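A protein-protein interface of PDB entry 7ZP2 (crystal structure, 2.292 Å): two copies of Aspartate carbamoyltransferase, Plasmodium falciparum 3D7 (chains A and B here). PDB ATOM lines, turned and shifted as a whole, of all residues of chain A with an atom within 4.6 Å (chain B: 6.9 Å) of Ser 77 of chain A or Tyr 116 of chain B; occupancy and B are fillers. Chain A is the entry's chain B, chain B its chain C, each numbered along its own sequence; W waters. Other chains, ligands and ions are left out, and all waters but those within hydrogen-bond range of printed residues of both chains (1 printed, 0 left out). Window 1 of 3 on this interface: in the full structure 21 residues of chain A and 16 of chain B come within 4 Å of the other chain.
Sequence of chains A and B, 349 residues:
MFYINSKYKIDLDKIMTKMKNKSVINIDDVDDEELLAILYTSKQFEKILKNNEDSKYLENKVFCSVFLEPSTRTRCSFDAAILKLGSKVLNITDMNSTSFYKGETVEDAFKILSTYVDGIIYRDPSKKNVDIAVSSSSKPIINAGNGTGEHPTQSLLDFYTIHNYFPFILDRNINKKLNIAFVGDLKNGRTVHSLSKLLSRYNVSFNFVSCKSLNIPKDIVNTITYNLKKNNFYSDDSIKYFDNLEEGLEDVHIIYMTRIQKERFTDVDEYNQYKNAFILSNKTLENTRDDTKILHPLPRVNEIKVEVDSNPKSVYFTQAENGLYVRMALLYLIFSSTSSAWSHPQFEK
Of the printed residues of chain A, Tyr 116 of chain B touches Arg 73 (3.5 Å), Ser 77 (3.8 Å), Ala 80 (3.5 Å) and Ala 320 (3.7 Å).
Of the printed residues of chain A, Leu 90 of chain B touches Cys 76 and Asp 79.
Printed residues of chain B within 4 Å of Ala 320 of chain A: Tyr 116.
Of the printed residues of chain A, Thr 115 of chain B touches Leu 324.
Cys 64 of chain B touches none of the printed residues of chain A.
The nearest printed residue of chain B that does not touch Ala 320 of chain A is Ile 112 of chain B (4.3 Å).
The side-chain carboxylate of Asp 79 of chain A lies within salt-bridge range of the guanidinium group of Arg 75 of chain A, at 2.7 Å.
OG of Ser 77 of chain A lies within hydrogen-bond range of NH1 of Arg 327 of chain A, 3.0 Å away.
O of Leu 90 of chain B sits close to SG of Cys 64 of chain B, 3.8 Å away.
The backbone carbonyl oxygen of Ile 112 of chain B lies within hydrogen-bond range of the side-chain hydroxyl of Thr 115 of chain B (2.5 Å).
Among the printed residues, merely in contact across the chains: Arg 73 of chain A with Ile 112 of chain B (3.3 Å), Ala 80 of chain A with Tyr 116 of chain B (3.5 Å), Arg 73 of chain A with Tyr 116 of chain B (3.5 Å), Asp 79 of chain A with Leu 90 of chain B (3.7 Å), Ala 320 of chain A with Tyr 116 of chain B (3.7 Å), Cys 76 of chain A with Leu 90 of chain B (3.7 Å), Ser 77 of chain A with Tyr 116 of chain B (3.8 Å) and Leu 324 of chain A with Thr 115 of chain B (3.9 Å).
Water W1 lies within hydrogen-bond range of NH1 of Arg 327 of chain A (2.7 Å), O of Ala 320 of chain A (2.9 Å) and OH of Tyr 116 of chain B (3.0 Å).
Printed residues of chain B that touch a printed residue of chain A: Leu 90, Ile 112, Thr 115 and Tyr 116.
Of the 13 printed residues of chain A, 7 touch a printed residue of chain B.
Hydrophobic or aromatic side chains of chain A within 4 Å of the printed part of chain B: Ala 80 and Leu 324.
Along chain A the printed residues that touch a printed residue of chain B span positions 73 to 324.
Among the printed residues, 8 pairs touch across the chains.
Among the printed residues, no Asp or Glu carboxylate lies within 4 Å of a Lys or Arg side-chain nitrogen of the other chain.
No position is printed for both chains.
Of the 8 pairs that touch across the chains among the printed residues, none has its exchanged pair printed and touching as well.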
ATOM      1  N   ARG A  73      12.265   2.301  -9.061  1.00  0.00           N
ATOM      2  CA  ARG A  73      13.194   1.550  -8.169  1.00  0.00           C
ATOM      3  C   ARG A  73      12.460   0.958  -6.972  1.00  0.00           C
ATOM      4  O   ARG A  73      12.791  -0.180  -6.600  1.00  0.00           O
ATOM      5  CB  ARG A  73      14.375   2.406  -7.704  1.00  0.00           C
ATOM      6  CG  ARG A  73      14.788   2.472  -6.234  1.00  0.00           C
ATOM      7  CD  ARG A  73      15.530   3.814  -5.956  1.00  0.00           C
ATOM      8  NE  ARG A  73      16.657   3.994  -6.860  1.00  0.00           N
ATOM      9  CZ  ARG A  73      16.665   4.722  -7.986  1.00  0.00           C
ATOM     10  NH1 ARG A  73      17.753   4.726  -8.779  1.00  0.00           N
ATOM     11  NH2 ARG A  73      15.597   5.444  -8.312  1.00  0.00           N
ATOM     12  N   THR A  74      11.607   1.732  -6.297  1.00  0.00           N
ATOM     13  CA  THR A  74      10.914   1.269  -5.084  1.00  0.00           C
ATOM     14  C   THR A  74       9.966   0.136  -5.530  1.00  0.00           C
ATOM     15  O   THR A  74       9.933  -0.874  -4.877  1.00  0.00           O
ATOM     16  CB  THR A  74      10.208   2.430  -4.365  1.00  0.00           C
ATOM     17  OG1 THR A  74      11.152   3.309  -3.795  1.00  0.00           O
ATOM     18  CG2 THR A  74       9.341   1.998  -3.220  1.00  0.00           C
ATOM     19  N   ARG A  75       9.302   0.302  -6.666  1.00  0.00           N
ATOM     20  CA  ARG A  75       8.291  -0.677  -7.135  1.00  0.00           C
ATOM     21  C   ARG A  75       8.976  -2.006  -7.502  1.00  0.00           C
ATOM     22  O   ARG A  75       8.489  -3.097  -7.053  1.00  0.00           O
ATOM     23  CB  ARG A  75       7.508  -0.068  -8.298  1.00  0.00           C
ATOM     24  CG  ARG A  75       6.494  -1.030  -8.931  1.00  0.00           C
ATOM     25  CD  ARG A  75       6.684  -0.837 -10.455  1.00  0.00           C
ATOM     26  NE  ARG A  75       6.937  -2.172 -10.850  1.00  0.00           N
ATOM     27  CZ  ARG A  75       6.964  -2.666 -12.029  1.00  0.00           C
ATOM     28  NH1 ARG A  75       7.211  -3.965 -12.128  1.00  0.00           N
ATOM     29  NH2 ARG A  75       6.771  -1.914 -13.070  1.00  0.00           N
ATOM     30  N   CYS A  76      10.063  -1.945  -8.274  1.00  0.00           N
ATOM     31  CA  CYS A  76      10.861  -3.111  -8.736  1.00  0.00           C
ATOM     32  C   CYS A  76      11.506  -3.835  -7.552  1.00  0.00           C
ATOM     33  O   CYS A  76      11.549  -5.077  -7.529  1.00  0.00           O
ATOM     34  CB  CYS A  76      11.902  -2.652  -9.732  1.00  0.00           C
ATOM     35  SG  CYS A  76      11.076  -2.186 -11.261  1.00  0.00           S
ATOM     36  N   SER A  77      11.953  -3.081  -6.566  1.00  0.00           N
ATOM     37  CA  SER A  77      12.585  -3.568  -5.316  1.00  0.00           C
ATOM     38  C   SER A  77      11.563  -4.365  -4.511  1.00  0.00           C
ATOM     39  O   SER A  77      11.853  -5.427  -3.969  1.00  0.00           O
ATOM     40  CB  SER A  77      13.044  -2.349  -4.573  1.00  0.00           C
ATOM     41  OG  SER A  77      13.734  -2.669  -3.426  1.00  0.00           O
ATOM     42  N   PHE A  78      10.373  -3.852  -4.368  1.00  0.00           N
ATOM     43  CA  PHE A  78       9.261  -4.608  -3.725  1.00  0.00           C
ATOM     44  C   PHE A  78       8.880  -5.841  -4.544  1.00  0.00           C
ATOM     45  O   PHE A  78       8.780  -6.919  -3.953  1.00  0.00           O
ATOM     46  CB  PHE A  78       8.118  -3.664  -3.470  1.00  0.00           C
ATOM     47  CG  PHE A  78       8.147  -2.964  -2.147  1.00  0.00           C
ATOM     48  CD1 PHE A  78       7.961  -3.645  -0.985  1.00  0.00           C
ATOM     49  CD2 PHE A  78       8.295  -1.592  -2.086  1.00  0.00           C
ATOM     50  CE1 PHE A  78       7.959  -2.964   0.218  1.00  0.00           C
ATOM     51  CE2 PHE A  78       8.197  -0.902  -0.907  1.00  0.00           C
ATOM     52  CZ  PHE A  78       8.092  -1.602   0.255  1.00  0.00           C
ATOM     53  N   ASP A  79       8.810  -5.755  -5.857  1.00  0.00           N
ATOM     54  CA  ASP A  79       8.528  -6.942  -6.723  1.00  0.00           C
ATOM     55  C   ASP A  79       9.578  -8.025  -6.485  1.00  0.00           C
ATOM     56  O   ASP A  79       9.228  -9.203  -6.270  1.00  0.00           O
ATOM     57  CB  ASP A  79       8.474  -6.610  -8.217  1.00  0.00           C
ATOM     58  CG  ASP A  79       7.166  -5.961  -8.691  1.00  0.00           C
ATOM     59  OD1 ASP A  79       6.142  -5.948  -7.878  1.00  0.00           O
ATOM     60  OD2 ASP A  79       7.151  -5.468  -9.882  1.00  0.00           O
ATOM     61  N   ALA A  80      10.842  -7.657  -6.649  1.00  0.00           N
ATOM     62  CA  ALA A  80      11.993  -8.558  -6.547  1.00  0.00           C
ATOM     63  C   ALA A  80      11.950  -9.227  -5.195  1.00  0.00           C
ATOM     64  O   ALA A  80      12.151 -10.437  -5.126  1.00  0.00           O
ATOM     65  CB  ALA A  80      13.270  -7.795  -6.760  1.00  0.00           C
ATOM     66  N   ALA A  81      11.656  -8.465  -4.164  1.00  0.00           N
ATOM     67  CA  ALA A  81      11.647  -8.976  -2.785  1.00  0.00           C
ATOM     68  C   ALA A  81      10.621 -10.077  -2.644  1.00  0.00           C
ATOM     69  O   ALA A  81      10.925 -11.172  -2.094  1.00  0.00           O
ATOM     70  CB  ALA A  81      11.399  -7.833  -1.818  1.00  0.00           C
ATOM     71  N   ALA A 320      20.957   1.455  -2.124  1.00  0.00           N
ATOM     72  CA  ALA A 320      19.820   1.135  -2.993  1.00  0.00           C
ATOM     73  C   ALA A 320      19.672  -0.379  -3.063  1.00  0.00           C
ATOM     74  O   ALA A 320      18.522  -0.859  -2.969  1.00  0.00           O
ATOM     75  CB  ALA A 320      19.988   1.689  -4.368  1.00  0.00           C
ATOM     76  N   GLY A 323      17.845  -1.972  -0.006  1.00  0.00           N
ATOM     77  CA  GLY A 323      16.377  -1.976  -0.028  1.00  0.00           C
ATOM     78  C   GLY A 323      15.801  -3.339  -0.355  1.00  0.00           C
ATOM     79  O   GLY A 323      14.727  -3.627   0.138  1.00  0.00           O
ATOM     80  N   LEU A 324      16.426  -4.123  -1.204  1.00  0.00           N
ATOM     81  CA  LEU A 324      15.964  -5.524  -1.498  1.00  0.00           C
ATOM     82  C   LEU A 324      15.923  -6.302  -0.169  1.00  0.00           C
ATOM     83  O   LEU A 324      14.884  -6.903   0.145  1.00  0.00           O
ATOM     84  CB  LEU A 324      16.853  -6.143  -2.579  1.00  0.00           C
ATOM     85  CG  LEU A 324      16.560  -7.640  -2.828  1.00  0.00           C
ATOM     86  CD1 LEU A 324      15.110  -7.794  -3.319  1.00  0.00           C
ATOM     87  CD2 LEU A 324      17.538  -8.255  -3.763  1.00  0.00           C
ATOM     88  N   ARG A 327      13.320  -4.906   2.421  1.00  0.00           N
ATOM     89  CA  ARG A 327      11.927  -5.248   1.986  1.00  0.00           C
ATOM     90  C   ARG A 327      11.684  -6.743   2.119  1.00  0.00           C
ATOM     91  O   ARG A 327      10.611  -7.073   2.616  1.00  0.00           O
ATOM     92  CB  ARG A 327      11.637  -4.576   0.652  1.00  0.00           C
ATOM     93  CG  ARG A 327      11.822  -3.078   0.781  1.00  0.00           C
ATOM     94  CD  ARG A 327      11.141  -2.031  -0.050  1.00  0.00           C
ATOM     95  NE  ARG A 327      12.060  -1.453  -0.846  1.00  0.00           N
ATOM     96  CZ  ARG A 327      12.525  -0.196  -0.993  1.00  0.00           C
ATOM     97  NH1 ARG A 327      13.464  -0.030  -1.923  1.00  0.00           N
ATOM     98  NH2 ARG A 327      12.096   0.827  -0.339  1.00  0.00           N
ATOM     99  N   VAL B  62      14.879 -14.890 -10.786  1.00  0.00           N
ATOM    100  CA  VAL B  62      14.021 -13.687 -10.850  1.00  0.00           C
ATOM    101  C   VAL B  62      14.639 -12.764 -11.878  1.00  0.00           C
ATOM    102  O   VAL B  62      15.846 -12.458 -11.748  1.00  0.00           O
ATOM    103  CB  VAL B  62      13.965 -13.020  -9.465  1.00  0.00           C
ATOM    104  CG1 VAL B  62      13.138 -11.749  -9.481  1.00  0.00           C
ATOM    105  CG2 VAL B  62      13.446 -14.016  -8.422  1.00  0.00           C
ATOM    106  N   CYS B  64      14.247  -9.283 -14.601  1.00  0.00           N
ATOM    107  CA  CYS B  64      13.616  -8.007 -14.945  1.00  0.00           C
ATOM    108  C   CYS B  64      13.567  -7.921 -16.472  1.00  0.00           C
ATOM    109  O   CYS B  64      14.561  -8.199 -17.141  1.00  0.00           O
ATOM    110  CB  CYS B  64      14.314  -6.811 -14.356  1.00  0.00           C
ATOM    111  SG  CYS B  64      13.390  -5.297 -14.660  1.00  0.00           S
ATOM    112  N   LEU B  90       9.704  -9.568 -13.127  1.00  0.00           N
ATOM    113  CA  LEU B  90       9.015  -8.254 -12.991  1.00  0.00           C
ATOM    114  C   LEU B  90       9.226  -7.513 -14.339  1.00  0.00           C
ATOM    115  O   LEU B  90      10.393  -7.580 -14.932  1.00  0.00           O
ATOM    116  CB  LEU B  90       9.569  -7.466 -11.795  1.00  0.00           C
ATOM    117  CG  LEU B  90      11.098  -7.401 -11.650  1.00  0.00           C
ATOM    118  CD1 LEU B  90      11.641  -6.013 -11.310  1.00  0.00           C
ATOM    119  CD2 LEU B  90      11.542  -8.380 -10.598  1.00  0.00           C
ATOM    120  N   LYS B 111      23.005  -0.172 -13.026  1.00  0.00           N
ATOM    121  CA  LYS B 111      23.852  -0.599 -11.890  1.00  0.00           C
ATOM    122  C   LYS B 111      22.932  -1.011 -10.727  1.00  0.00           C
ATOM    123  O   LYS B 111      23.232  -2.013 -10.027  1.00  0.00           O
ATOM    124  CB  LYS B 111      24.864   0.500 -11.545  1.00  0.00           C
ATOM    125  CG  LYS B 111      25.874   0.138 -10.474  1.00  0.00           C
ATOM    126  CD  LYS B 111      27.270   0.672 -10.645  1.00  0.00           C
ATOM    127  CE  LYS B 111      28.140   0.376  -9.441  1.00  0.00           C
ATOM    128  NZ  LYS B 111      28.448  -1.068  -9.239  1.00  0.00           N
ATOM    129  N   ILE B 112      21.861  -0.280 -10.541  1.00  0.00           N
ATOM    130  CA  ILE B 112      20.910  -0.486  -9.410  1.00  0.00           C
ATOM    131  C   ILE B 112      20.006  -1.678  -9.739  1.00  0.00           C
ATOM    132  O   ILE B 112      19.924  -2.619  -8.935  1.00  0.00           O
ATOM    133  CB  ILE B 112      20.096   0.797  -9.166  1.00  0.00           C
ATOM    134  CG1 ILE B 112      20.981   1.850  -8.518  1.00  0.00           C
ATOM    135  CG2 ILE B 112      18.848   0.550  -8.336  1.00  0.00           C
ATOM    136  CD1 ILE B 112      20.672   3.257  -8.939  1.00  0.00           C
ATOM    137  N   LEU B 113      19.405  -1.661 -10.926  1.00  0.00           N
ATOM    138  CA  LEU B 113      18.413  -2.686 -11.248  1.00  0.00           C
ATOM    139  C   LEU B 113      19.051  -4.086 -11.161  1.00  0.00           C
ATOM    140  O   LEU B 113      18.341  -5.049 -10.722  1.00  0.00           O
ATOM    141  CB  LEU B 113      17.885  -2.354 -12.632  1.00  0.00           C
ATOM    142  CG  LEU B 113      16.831  -3.296 -13.167  1.00  0.00           C
ATOM    143  CD1 LEU B 113      15.600  -3.272 -12.197  1.00  0.00           C
ATOM    144  CD2 LEU B 113      16.511  -2.857 -14.583  1.00  0.00           C
ATOM    145  N   SER B 114      20.318  -4.208 -11.525  1.00  0.00           N
ATOM    146  CA  SER B 114      20.989  -5.520 -11.631  1.00  0.00           C
ATOM    147  C   SER B 114      21.285  -6.057 -10.227  1.00  0.00           C
ATOM    148  O   SER B 114      21.541  -7.258 -10.119  1.00  0.00           O
ATOM    149  CB  SER B 114      22.203  -5.489 -12.529  1.00  0.00           C
ATOM    150  OG  SER B 114      23.088  -4.468 -12.168  1.00  0.00           O
ATOM    151  N   THR B 115      21.186  -5.212  -9.185  1.00  0.00           N
ATOM    152  CA  THR B 115      21.358  -5.679  -7.786  1.00  0.00           C
ATOM    153  C   THR B 115      20.083  -6.445  -7.398  1.00  0.00           C
ATOM    154  O   THR B 115      20.191  -7.300  -6.527  1.00  0.00           O
ATOM    155  CB  THR B 115      21.791  -4.524  -6.886  1.00  0.00           C
ATOM    156  OG1 THR B 115      20.811  -3.479  -6.766  1.00  0.00           O
ATOM    157  CG2 THR B 115      23.097  -3.924  -7.375  1.00  0.00           C
ATOM    158  N   TYR B 116      18.953  -6.260  -8.081  1.00  0.00           N
ATOM    159  CA  TYR B 116      17.663  -6.804  -7.627  1.00  0.00           C
ATOM    160  C   TYR B 116      17.438  -8.207  -8.154  1.00  0.00           C
ATOM    161  O   TYR B 116      16.531  -8.809  -7.614  1.00  0.00           O
ATOM    162  CB  TYR B 116      16.456  -5.965  -8.084  1.00  0.00           C
ATOM    163  CG  TYR B 116      16.387  -4.555  -7.532  1.00  0.00           C
ATOM    164  CD1 TYR B 116      17.108  -4.214  -6.417  1.00  0.00           C
ATOM    165  CD2 TYR B 116      15.611  -3.583  -8.133  1.00  0.00           C
ATOM    166  CE1 TYR B 116      17.032  -2.947  -5.865  1.00  0.00           C
ATOM    167  CE2 TYR B 116      15.577  -2.284  -7.647  1.00  0.00           C
ATOM    168  CZ  TYR B 116      16.329  -1.950  -6.522  1.00  0.00           C
ATOM    169  OH  TYR B 116      16.368  -0.676  -5.992  1.00  0.00           O
ATOM    170  N   VAL B 117      18.107  -8.623  -9.239  1.00  0.00           N
ATOM    171  CA  VAL B 117      17.601  -9.683 -10.155  1.00  0.00           C
ATOM    172  C   VAL B 117      18.795 -10.460 -10.680  1.00  0.00           C
ATOM    173  O   VAL B 117      19.857  -9.998 -10.548  1.00  0.00           O
ATOM    174  CB  VAL B 117      16.753  -9.122 -11.325  1.00  0.00           C
ATOM    175  CG1 VAL B 117      15.484  -8.506 -10.811  1.00  0.00           C
ATOM    176  CG2 VAL B 117      17.538  -8.136 -12.179  1.00  0.00           C
ATOM    177  N   ASP B 118      18.527 -11.597 -11.324  1.00  0.00           N
ATOM    178  CA  ASP B 118      19.558 -12.561 -11.824  1.00  0.00           C
ATOM    179  C   ASP B 118      19.905 -12.239 -13.265  1.00  0.00           C
ATOM    180  O   ASP B 118      20.985 -12.607 -13.759  1.00  0.00           O
ATOM    181  CB  ASP B 118      19.057 -13.993 -11.662  1.00  0.00           C
ATOM    182  CG  ASP B 118      18.734 -14.298 -10.209  1.00  0.00           C
ATOM    183  OD1 ASP B 118      19.529 -13.883  -9.272  1.00  0.00           O
ATOM    184  OD2 ASP B 118      17.632 -14.761  -9.965  1.00  0.00           O
ATOM    185  N   GLY B 119      19.047 -11.498 -13.945  1.00  0.00           N
ATOM    186  CA  GLY B 119      19.231 -11.219 -15.382  1.00  0.00           C
ATOM    187  C   GLY B 119      18.197 -10.247 -15.873  1.00  0.00           C
ATOM    188  O   GLY B 119      17.189 -10.078 -15.242  1.00  0.00           O
ATOM    189  N   SER B 138      25.738  -5.547 -13.323  1.00  0.00           N
ATOM    190  CA  SER B 138      26.469  -6.668 -12.687  1.00  0.00           C
ATOM    191  C   SER B 138      25.895  -7.997 -13.159  1.00  0.00           C
ATOM    192  O   SER B 138      26.437  -9.066 -12.802  1.00  0.00           O
ATOM    193  CB  SER B 138      26.462  -6.540 -11.169  1.00  0.00           C
ATOM    194  OG  SER B 138      25.137  -6.369 -10.706  1.00  0.00           O
ATOM    195  N   LYS B 139      24.816  -7.991 -13.944  1.00  0.00           N
ATOM    196  CA  LYS B 139      24.161  -9.260 -14.349  1.00  0.00           C
ATOM    197  C   LYS B 139      24.035  -9.336 -15.860  1.00  0.00           C
ATOM    198  O   LYS B 139      23.940  -8.314 -16.532  1.00  0.00           O
ATOM    199  CB  LYS B 139      22.780  -9.369 -13.714  1.00  0.00           C
ATOM    200  CG  LYS B 139      22.772  -9.350 -12.196  1.00  0.00           C
ATOM    201  CD  LYS B 139      23.352 -10.645 -11.607  1.00  0.00           C
ATOM    202  CE  LYS B 139      23.752 -10.495 -10.158  1.00  0.00           C
ATOM    203  NZ  LYS B 139      22.682  -9.779  -9.384  1.00  0.00           N
HETATM  204  O   HOH W   1      15.787   0.177  -3.223  1.00  0.00           O
